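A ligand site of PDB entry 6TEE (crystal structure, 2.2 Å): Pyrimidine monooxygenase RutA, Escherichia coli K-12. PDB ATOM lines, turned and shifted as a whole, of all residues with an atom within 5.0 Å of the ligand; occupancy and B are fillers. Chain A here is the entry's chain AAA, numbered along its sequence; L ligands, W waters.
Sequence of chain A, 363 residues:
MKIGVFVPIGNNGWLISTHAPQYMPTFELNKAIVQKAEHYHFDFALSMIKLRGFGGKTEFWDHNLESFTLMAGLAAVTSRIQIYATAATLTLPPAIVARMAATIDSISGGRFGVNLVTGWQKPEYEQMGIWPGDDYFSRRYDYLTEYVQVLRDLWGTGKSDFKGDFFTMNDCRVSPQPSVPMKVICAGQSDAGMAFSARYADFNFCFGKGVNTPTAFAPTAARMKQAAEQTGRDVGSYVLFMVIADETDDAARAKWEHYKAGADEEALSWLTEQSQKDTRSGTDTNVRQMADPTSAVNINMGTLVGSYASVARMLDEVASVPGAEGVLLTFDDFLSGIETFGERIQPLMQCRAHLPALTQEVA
An oxygen (O8) of the ligand is in hydrogen-bond range of the side-chain hydroxyl (OH) of Tyr 141, at 2.7 Å.
The backbone NH of Ser 190 sits at hydrogen-bond distance from an oxygen (O9) of the ligand, at 3.1 Å.
The side-chain hydroxyl (OG) of Ser 190 is in hydrogen-bond range of an oxygen (O9) of the ligand.
An oxygen (O7) of the ligand is in salt-bridge range of the guanidinium group of Arg 140.
The backbone NH (N) of Ile 49 sits at hydrogen-bond distance from an oxygen (O2) of the ligand (2.8 Å).
N2 of the ligand lies within hydrogen-bond range of O of Ile 49 (3.3 Å).
O5 of the ligand lies within hydrogen-bond range of O of Ala 187 (3.0 Å).
The backbone NH (N) of Gln 189 sits at hydrogen-bond distance from an oxygen (O9) of the ligand, 3.0 Å away.
OG of Ser 190 is in hydrogen-bond range of N of Gly 193, 3.1 Å away.
NH2 of Arg 140 sits at hydrogen-bond distance from OG1 of Thr 118.
O of Ala 187 lies close to OE1 of Gln 189, 3.2 Å away.
The backbone carbonyl oxygen (O) of Phe 205 sits close to the side-chain amide oxygen (OE1) of Gln 189, 3.1 Å away.
The side-chain hydroxyl (OG1) of Thr 86 is in hydrogen-bond range of the side-chain amide nitrogen (ND2) of Asn 115 (3.1 Å).
Merely in contact with the ligand: Met 48, Val 117, Thr 86, Gly 188, Trp 120, Phe 6, Gly 193, Phe 207, Leu 328, Gly 119 and Phe 205.
Of the 23 residues printed, 17 come within 4 Å of the ligand.
Water W2 lies within hydrogen-bond range of OH of Tyr 125 (2.4 Å) and O1 of the ligand (2.7 Å).
Water W3 lies within hydrogen-bond range of O3 of the ligand, N of Thr 118 and OH of Tyr 141.
Water W1 lies within hydrogen-bond range of N of Gly 119, O4 of the ligand and N of Thr 118.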
ATOM      1  N   PHE A   6       7.206 -16.633  17.916  1.00  0.00           N
ATOM      2  CA  PHE A   6       7.748 -17.339  19.064  1.00  0.00           C
ATOM      3  C   PHE A   6       9.126 -16.730  19.359  1.00  0.00           C
ATOM      4  O   PHE A   6      10.094 -16.954  18.620  1.00  0.00           O
ATOM      5  CB  PHE A   6       7.770 -18.832  18.708  1.00  0.00           C
ATOM      6  CG  PHE A   6       7.596 -19.853  19.797  1.00  0.00           C
ATOM      7  CD1 PHE A   6       7.184 -19.508  21.091  1.00  0.00           C
ATOM      8  CD2 PHE A   6       7.819 -21.206  19.521  1.00  0.00           C
ATOM      9  CE1 PHE A   6       7.042 -20.487  22.074  1.00  0.00           C
ATOM     10  CE2 PHE A   6       7.657 -22.183  20.503  1.00  0.00           C
ATOM     11  CZ  PHE A   6       7.289 -21.819  21.782  1.00  0.00           C
ATOM     12  N   LEU A  46       4.748 -14.593  21.706  1.00  0.00           N
ATOM     13  CA  LEU A  46       4.739 -15.591  22.777  1.00  0.00           C
ATOM     14  C   LEU A  46       6.174 -15.961  23.142  1.00  0.00           C
ATOM     15  O   LEU A  46       6.970 -16.290  22.258  1.00  0.00           O
ATOM     16  CB  LEU A  46       4.012 -16.844  22.272  1.00  0.00           C
ATOM     17  CG  LEU A  46       4.141 -18.074  23.166  1.00  0.00           C
ATOM     18  CD1 LEU A  46       3.454 -17.904  24.518  1.00  0.00           C
ATOM     19  CD2 LEU A  46       3.637 -19.345  22.485  1.00  0.00           C
ATOM     20  N   MET A  48       8.046 -19.065  25.474  1.00  0.00           N
ATOM     21  CA  MET A  48       8.072 -20.274  26.290  1.00  0.00           C
ATOM     22  C   MET A  48       8.831 -20.018  27.591  1.00  0.00           C
ATOM     23  O   MET A  48       9.339 -18.918  27.826  1.00  0.00           O
ATOM     24  CB  MET A  48       8.726 -21.435  25.542  1.00  0.00           C
ATOM     25  CG  MET A  48      10.181 -21.198  25.190  1.00  0.00           C
ATOM     26  SD  MET A  48      11.148 -22.704  24.860  1.00  0.00           S
ATOM     27  CE  MET A  48      12.753 -21.947  24.630  1.00  0.00           C
ATOM     28  N   ILE A  49       8.884 -21.048  28.449  1.00  0.00           N
ATOM     29  CA  ILE A  49       9.768 -21.122  29.608  1.00  0.00           C
ATOM     30  C   ILE A  49      10.504 -22.472  29.500  1.00  0.00           C
ATOM     31  O   ILE A  49       9.865 -23.508  29.356  1.00  0.00           O
ATOM     32  CB  ILE A  49       8.978 -20.986  30.924  1.00  0.00           C
ATOM     33  CG1 ILE A  49       9.864 -20.968  32.189  1.00  0.00           C
ATOM     34  CG2 ILE A  49       7.873 -22.050  31.042  1.00  0.00           C
ATOM     35  CD1 ILE A  49      10.659 -19.688  32.375  1.00  0.00           C
ATOM     36  N   THR A  86       4.421 -17.667  29.341  1.00  0.00           N
ATOM     37  CA  THR A  86       4.157 -19.032  29.765  1.00  0.00           C
ATOM     38  C   THR A  86       4.381 -19.171  31.278  1.00  0.00           C
ATOM     39  O   THR A  86       5.441 -18.816  31.803  1.00  0.00           O
ATOM     40  CB  THR A  86       5.019 -20.048  29.006  1.00  0.00           C
ATOM     41  OG1 THR A  86       4.869 -19.803  27.600  1.00  0.00           O
ATOM     42  CG2 THR A  86       4.588 -21.480  29.269  1.00  0.00           C
ATOM     43  N   ASN A 115      -0.008 -18.429  28.749  1.00  0.00           N
ATOM     44  CA  ASN A 115       0.010 -19.797  28.223  1.00  0.00           C
ATOM     45  C   ASN A 115       0.293 -20.731  29.395  1.00  0.00           C
ATOM     46  O   ASN A 115       1.312 -20.552  30.063  1.00  0.00           O
ATOM     47  CB  ASN A 115       0.988 -19.877  27.039  1.00  0.00           C
ATOM     48  CG  ASN A 115       1.314 -21.273  26.544  1.00  0.00           C
ATOM     49  OD1 ASN A 115       0.441 -22.095  26.330  1.00  0.00           O
ATOM     50  ND2 ASN A 115       2.603 -21.516  26.340  1.00  0.00           N
ATOM     51  N   VAL A 117       1.044 -24.310  31.029  1.00  0.00           N
ATOM     52  CA  VAL A 117       1.606 -25.612  30.762  1.00  0.00           C
ATOM     53  C   VAL A 117       1.752 -26.410  32.069  1.00  0.00           C
ATOM     54  O   VAL A 117       1.974 -25.854  33.163  1.00  0.00           O
ATOM     55  CB  VAL A 117       2.899 -25.512  29.939  1.00  0.00           C
ATOM     56  CG1 VAL A 117       2.662 -24.835  28.586  1.00  0.00           C
ATOM     57  CG2 VAL A 117       4.075 -24.871  30.686  1.00  0.00           C
ATOM     58  N   THR A 118       1.645 -27.743  31.931  1.00  0.00           N
ATOM     59  CA  THR A 118       1.793 -28.663  33.042  1.00  0.00           C
ATOM     60  C   THR A 118       3.273 -28.830  33.367  1.00  0.00           C
ATOM     61  O   THR A 118       3.651 -28.912  34.537  1.00  0.00           O
ATOM     62  CB  THR A 118       1.122 -30.013  32.722  1.00  0.00           C
ATOM     63  OG1 THR A 118       1.802 -30.623  31.623  1.00  0.00           O
ATOM     64  CG2 THR A 118      -0.365 -29.908  32.380  1.00  0.00           C
ATOM     65  N   GLY A 119       4.096 -28.856  32.306  1.00  0.00           N
ATOM     66  CA  GLY A 119       5.459 -29.365  32.351  1.00  0.00           C
ATOM     67  C   GLY A 119       5.466 -30.853  32.065  1.00  0.00           C
ATOM     68  O   GLY A 119       4.483 -31.541  32.325  1.00  0.00           O
ATOM     69  N   TRP A 120       6.560 -31.370  31.519  1.00  0.00           N
ATOM     70  CA  TRP A 120       6.598 -32.806  31.294  1.00  0.00           C
ATOM     71  C   TRP A 120       8.032 -33.326  31.458  1.00  0.00           C
ATOM     72  O   TRP A 120       8.236 -34.521  31.676  1.00  0.00           O
ATOM     73  CB  TRP A 120       5.928 -33.202  29.959  1.00  0.00           C
ATOM     74  CG  TRP A 120       6.534 -32.547  28.765  1.00  0.00           C
ATOM     75  CD1 TRP A 120       6.235 -31.314  28.257  1.00  0.00           C
ATOM     76  CD2 TRP A 120       7.606 -33.066  27.958  1.00  0.00           C
ATOM     77  NE1 TRP A 120       7.043 -31.034  27.179  1.00  0.00           N
ATOM     78  CE2 TRP A 120       7.888 -32.095  26.979  1.00  0.00           C
ATOM     79  CE3 TRP A 120       8.330 -34.261  27.972  1.00  0.00           C
ATOM     80  CZ2 TRP A 120       8.887 -32.283  26.025  1.00  0.00           C
ATOM     81  CZ3 TRP A 120       9.317 -34.451  27.031  1.00  0.00           C
ATOM     82  CH2 TRP A 120       9.590 -33.466  26.067  1.00  0.00           C
ATOM     83  N   TYR A 125      12.374 -29.951  36.828  1.00  0.00           N
ATOM     84  CA  TYR A 125      11.717 -29.825  38.112  1.00  0.00           C
ATOM     85  C   TYR A 125      12.515 -30.538  39.189  1.00  0.00           C
ATOM     86  O   TYR A 125      12.647 -30.049  40.308  1.00  0.00           O
ATOM     87  CB  TYR A 125      10.293 -30.369  37.994  1.00  0.00           C
ATOM     88  CG  TYR A 125       9.542 -29.552  36.965  1.00  0.00           C
ATOM     89  CD1 TYR A 125       9.146 -28.274  37.286  1.00  0.00           C
ATOM     90  CD2 TYR A 125       9.347 -30.007  35.658  1.00  0.00           C
ATOM     91  CE1 TYR A 125       8.497 -27.469  36.365  1.00  0.00           C
ATOM     92  CE2 TYR A 125       8.710 -29.207  34.716  1.00  0.00           C
ATOM     93  CZ  TYR A 125       8.267 -27.947  35.088  1.00  0.00           C
ATOM     94  OH  TYR A 125       7.628 -27.113  34.207  1.00  0.00           O
ATOM     95  N   ARG A 140      -1.572 -34.698  35.611  1.00  0.00           N
ATOM     96  CA  ARG A 140      -1.187 -33.293  35.519  1.00  0.00           C
ATOM     97  C   ARG A 140      -2.356 -32.387  35.088  1.00  0.00           C
ATOM     98  O   ARG A 140      -2.396 -31.219  35.476  1.00  0.00           O
ATOM     99  CB  ARG A 140       0.100 -33.150  34.702  1.00  0.00           C
ATOM    100  CG  ARG A 140      -0.004 -33.683  33.278  1.00  0.00           C
ATOM    101  CD  ARG A 140       1.352 -34.035  32.706  1.00  0.00           C
ATOM    102  NE  ARG A 140       1.230 -34.730  31.416  1.00  0.00           N
ATOM    103  CZ  ARG A 140       1.224 -34.148  30.206  1.00  0.00           C
ATOM    104  NH1 ARG A 140       1.111 -34.888  29.125  1.00  0.00           N
ATOM    105  NH2 ARG A 140       1.360 -32.828  30.080  1.00  0.00           N
ATOM    106  N   TYR A 141      -3.303 -32.914  34.291  1.00  0.00           N
ATOM    107  CA  TYR A 141      -4.455 -32.154  33.820  1.00  0.00           C
ATOM    108  C   TYR A 141      -5.484 -31.945  34.946  1.00  0.00           C
ATOM    109  O   TYR A 141      -6.140 -30.899  35.018  1.00  0.00           O
ATOM    110  CB  TYR A 141      -4.906 -32.544  32.392  1.00  0.00           C
ATOM    111  CG  TYR A 141      -4.000 -32.039  31.282  1.00  0.00           C
ATOM    112  CD1 TYR A 141      -3.976 -30.702  30.919  1.00  0.00           C
ATOM    113  CD2 TYR A 141      -3.136 -32.900  30.596  1.00  0.00           C
ATOM    114  CE1 TYR A 141      -3.112 -30.213  29.947  1.00  0.00           C
ATOM    115  CE2 TYR A 141      -2.274 -32.437  29.605  1.00  0.00           C
ATOM    116  CZ  TYR A 141      -2.241 -31.079  29.288  1.00  0.00           C
ATOM    117  OH  TYR A 141      -1.389 -30.609  28.305  1.00  0.00           O
ATOM    118  N   ALA A 187      -1.320 -25.689  25.111  1.00  0.00           N
ATOM    119  CA  ALA A 187      -0.561 -26.360  24.083  1.00  0.00           C
ATOM    120  C   ALA A 187      -0.700 -27.894  24.208  1.00  0.00           C
ATOM    121  O   ALA A 187       0.210 -28.641  23.885  1.00  0.00           O
ATOM    122  CB  ALA A 187       0.871 -25.879  24.136  1.00  0.00           C
ATOM    123  N   GLY A 188      -1.876 -28.374  24.652  1.00  0.00           N
ATOM    124  CA  GLY A 188      -2.068 -29.814  24.807  1.00  0.00           C
ATOM    125  C   GLY A 188      -2.302 -30.543  23.480  1.00  0.00           C
ATOM    126  O   GLY A 188      -3.039 -30.034  22.631  1.00  0.00           O
ATOM    127  N   GLN A 189      -1.676 -31.732  23.328  1.00  0.00           N
ATOM    128  CA  GLN A 189      -1.670 -32.505  22.096  1.00  0.00           C
ATOM    129  C   GLN A 189      -2.454 -33.800  22.296  1.00  0.00           C
ATOM    130  O   GLN A 189      -3.028 -34.335  21.353  1.00  0.00           O
ATOM    131  CB  GLN A 189      -0.272 -32.944  21.638  1.00  0.00           C
ATOM    132  CG  GLN A 189       0.752 -31.853  21.437  1.00  0.00           C
ATOM    133  CD  GLN A 189       0.309 -30.787  20.456  1.00  0.00           C
ATOM    134  OE1 GLN A 189      -0.032 -29.676  20.852  1.00  0.00           O
ATOM    135  NE2 GLN A 189       0.296 -31.133  19.167  1.00  0.00           N
ATOM    136  N   SER A 190      -2.412 -34.318  23.532  1.00  0.00           N
ATOM    137  CA  SER A 190      -3.100 -35.539  23.902  1.00  0.00           C
ATOM    138  C   SER A 190      -4.606 -35.287  24.038  1.00  0.00           C
ATOM    139  O   SER A 190      -5.081 -34.141  23.997  1.00  0.00           O
ATOM    140  CB  SER A 190      -2.547 -36.034  25.217  1.00  0.00           C
ATOM    141  OG  SER A 190      -2.890 -35.136  26.271  1.00  0.00           O
ATOM    142  N   GLY A 193      -5.169 -33.195  27.124  1.00  0.00           N
ATOM    143  CA  GLY A 193      -4.751 -31.806  26.968  1.00  0.00           C
ATOM    144  C   GLY A 193      -5.762 -31.022  26.140  1.00  0.00           C
ATOM    145  O   GLY A 193      -6.085 -29.889  26.469  1.00  0.00           O
ATOM    146  N   PHE A 205      -2.454 -24.327  20.855  1.00  0.00           N
ATOM    147  CA  PHE A 205      -1.270 -24.494  20.021  1.00  0.00           C
ATOM    148  C   PHE A 205      -1.022 -25.982  19.758  1.00  0.00           C
ATOM    149  O   PHE A 205      -1.049 -26.766  20.707  1.00  0.00           O
ATOM    150  CB  PHE A 205      -0.019 -23.944  20.698  1.00  0.00           C
ATOM    151  CG  PHE A 205       0.011 -22.443  20.773  1.00  0.00           C
ATOM    152  CD1 PHE A 205       0.083 -21.668  19.619  1.00  0.00           C
ATOM    153  CD2 PHE A 205      -0.049 -21.798  21.990  1.00  0.00           C
ATOM    154  CE1 PHE A 205       0.082 -20.288  19.660  1.00  0.00           C
ATOM    155  CE2 PHE A 205      -0.060 -20.417  22.031  1.00  0.00           C
ATOM    156  CZ  PHE A 205      -0.019 -19.659  20.864  1.00  0.00           C
ATOM    157  N   CYS A 206      -0.812 -26.308  18.477  1.00  0.00           N
ATOM    158  CA  CYS A 206      -0.330 -27.615  18.052  1.00  0.00           C
ATOM    159  C   CYS A 206       0.870 -27.444  17.102  1.00  0.00           C
ATOM    160  O   CYS A 206       1.186 -26.330  16.690  1.00  0.00           O
ATOM    161  CB  CYS A 206      -1.459 -28.411  17.395  1.00  0.00           C
ATOM    162  SG  CYS A 206      -1.981 -27.747  15.791  1.00  0.00           S
ATOM    163  N   PHE A 207       1.479 -28.576  16.719  1.00  0.00           N
ATOM    164  CA  PHE A 207       2.689 -28.665  15.927  1.00  0.00           C
ATOM    165  C   PHE A 207       2.366 -28.763  14.430  1.00  0.00           C
ATOM    166  O   PHE A 207       1.578 -29.600  14.013  1.00  0.00           O
ATOM    167  CB  PHE A 207       3.489 -29.899  16.344  1.00  0.00           C
ATOM    168  CG  PHE A 207       4.171 -29.770  17.678  1.00  0.00           C
ATOM    169  CD1 PHE A 207       5.223 -28.889  17.860  1.00  0.00           C
ATOM    170  CD2 PHE A 207       3.735 -30.500  18.777  1.00  0.00           C
ATOM    171  CE1 PHE A 207       5.805 -28.716  19.112  1.00  0.00           C
ATOM    172  CE2 PHE A 207       4.343 -30.364  20.019  1.00  0.00           C
ATOM    173  CZ  PHE A 207       5.369 -29.458  20.195  1.00  0.00           C
ATOM    174  N   LEU A 240       2.452 -24.286  14.939  1.00  0.00           N
ATOM    175  CA  LEU A 240       3.846 -23.855  15.017  1.00  0.00           C
ATOM    176  C   LEU A 240       4.624 -24.323  13.775  1.00  0.00           C
ATOM    177  O   LEU A 240       4.665 -25.518  13.469  1.00  0.00           O
ATOM    178  CB  LEU A 240       4.498 -24.390  16.299  1.00  0.00           C
ATOM    179  CG  LEU A 240       6.019 -24.225  16.437  1.00  0.00           C
ATOM    180  CD1 LEU A 240       6.451 -22.760  16.487  1.00  0.00           C
ATOM    181  CD2 LEU A 240       6.513 -24.934  17.688  1.00  0.00           C
ATOM    182  N   LEU A 328       2.018 -19.934  14.659  1.00  0.00           N
ATOM    183  CA  LEU A 328       3.089 -19.379  15.471  1.00  0.00           C
ATOM    184  C   LEU A 328       4.417 -19.627  14.746  1.00  0.00           C
ATOM    185  O   LEU A 328       4.712 -20.776  14.355  1.00  0.00           O
ATOM    186  CB  LEU A 328       3.021 -20.064  16.846  1.00  0.00           C
ATOM    187  CG  LEU A 328       4.151 -19.693  17.795  1.00  0.00           C
ATOM    188  CD1 LEU A 328       4.129 -18.205  18.144  1.00  0.00           C
ATOM    189  CD2 LEU A 328       4.153 -20.579  19.020  1.00  0.00           C
HETATM  190  N1  LIG L   1       5.965 -26.927  27.725  1.00  0.00           N
HETATM  191  C1  LIG L   1       6.621 -26.319  28.751  1.00  0.00           C
HETATM  192  O1  LIG L   1       6.859 -27.038  29.762  1.00  0.00           O
HETATM  193  N2  LIG L   1       6.983 -25.004  28.701  1.00  0.00           N
HETATM  194  C2  LIG L   1       6.716 -24.223  27.632  1.00  0.00           C
HETATM  195  O2  LIG L   1       7.043 -23.012  27.622  1.00  0.00           O
HETATM  196  C3  LIG L   1       5.996 -24.850  26.483  1.00  0.00           C
HETATM  197  N3  LIG L   1       5.681 -24.148  25.399  1.00  0.00           N
HETATM  198  C4  LIG L   1       5.054 -24.765  24.367  1.00  0.00           C
HETATM  199  C5  LIG L   1       4.759 -24.001  23.236  1.00  0.00           C
HETATM  200  C6  LIG L   1       4.138 -24.603  22.143  1.00  0.00           C
HETATM  201  C7  LIG L   1       3.867 -23.736  20.984  1.00  0.00           C
HETATM  202  C8  LIG L   1       3.724 -26.044  22.163  1.00  0.00           C
HETATM  203  C9  LIG L   1       3.022 -26.705  20.990  1.00  0.00           C
HETATM  204  C10 LIG L   1       4.030 -26.814  23.273  1.00  0.00           C
HETATM  205  C11 LIG L   1       4.689 -26.230  24.367  1.00  0.00           C
HETATM  206  N4  LIG L   1       4.964 -26.987  25.505  1.00  0.00           N
HETATM  207  C12 LIG L   1       5.627 -26.292  26.579  1.00  0.00           C
HETATM  208  C13 LIG L   1       4.566 -28.412  25.601  1.00  0.00           C
HETATM  209  C14 LIG L   1       3.021 -28.538  25.845  1.00  0.00           C
HETATM  210  O3  LIG L   1       2.486 -27.643  26.903  1.00  0.00           O
HETATM  211  C15 LIG L   1       2.473 -29.995  26.016  1.00  0.00           C
HETATM  212  O4  LIG L   1       2.864 -30.518  27.290  1.00  0.00           O
HETATM  213  C16 LIG L   1       2.913 -31.011  24.961  1.00  0.00           C
HETATM  214  O5  LIG L   1       2.615 -30.486  23.659  1.00  0.00           O
HETATM  215  C17 LIG L   1       2.405 -32.478  25.126  1.00  0.00           C
HETATM  216  O6  LIG L   1       0.971 -32.673  24.984  1.00  0.00           O
HETATM  217  P1  LIG L   1       0.154 -33.036  26.336  1.00  0.00           P
HETATM  218  O7  LIG L   1       0.635 -34.472  26.395  1.00  0.00           O
HETATM  219  O8  LIG L   1       0.609 -32.114  27.416  1.00  0.00           O
HETATM  220  O9  LIG L   1      -1.328 -32.899  26.121  1.00  0.00           O
HETATM  221  O   HOH W   1       3.903 -28.775  29.612  1.00  0.00           O
HETATM  222  O   HOH W   2       8.442 -27.248  31.904  1.00  0.00           O
HETATM  223  O   HOH W   3       0.701 -28.377  29.041  1.00  0.00           O
HETATM  224  O   HOH W   4       1.135 -35.864  23.723  1.00  0.00           O
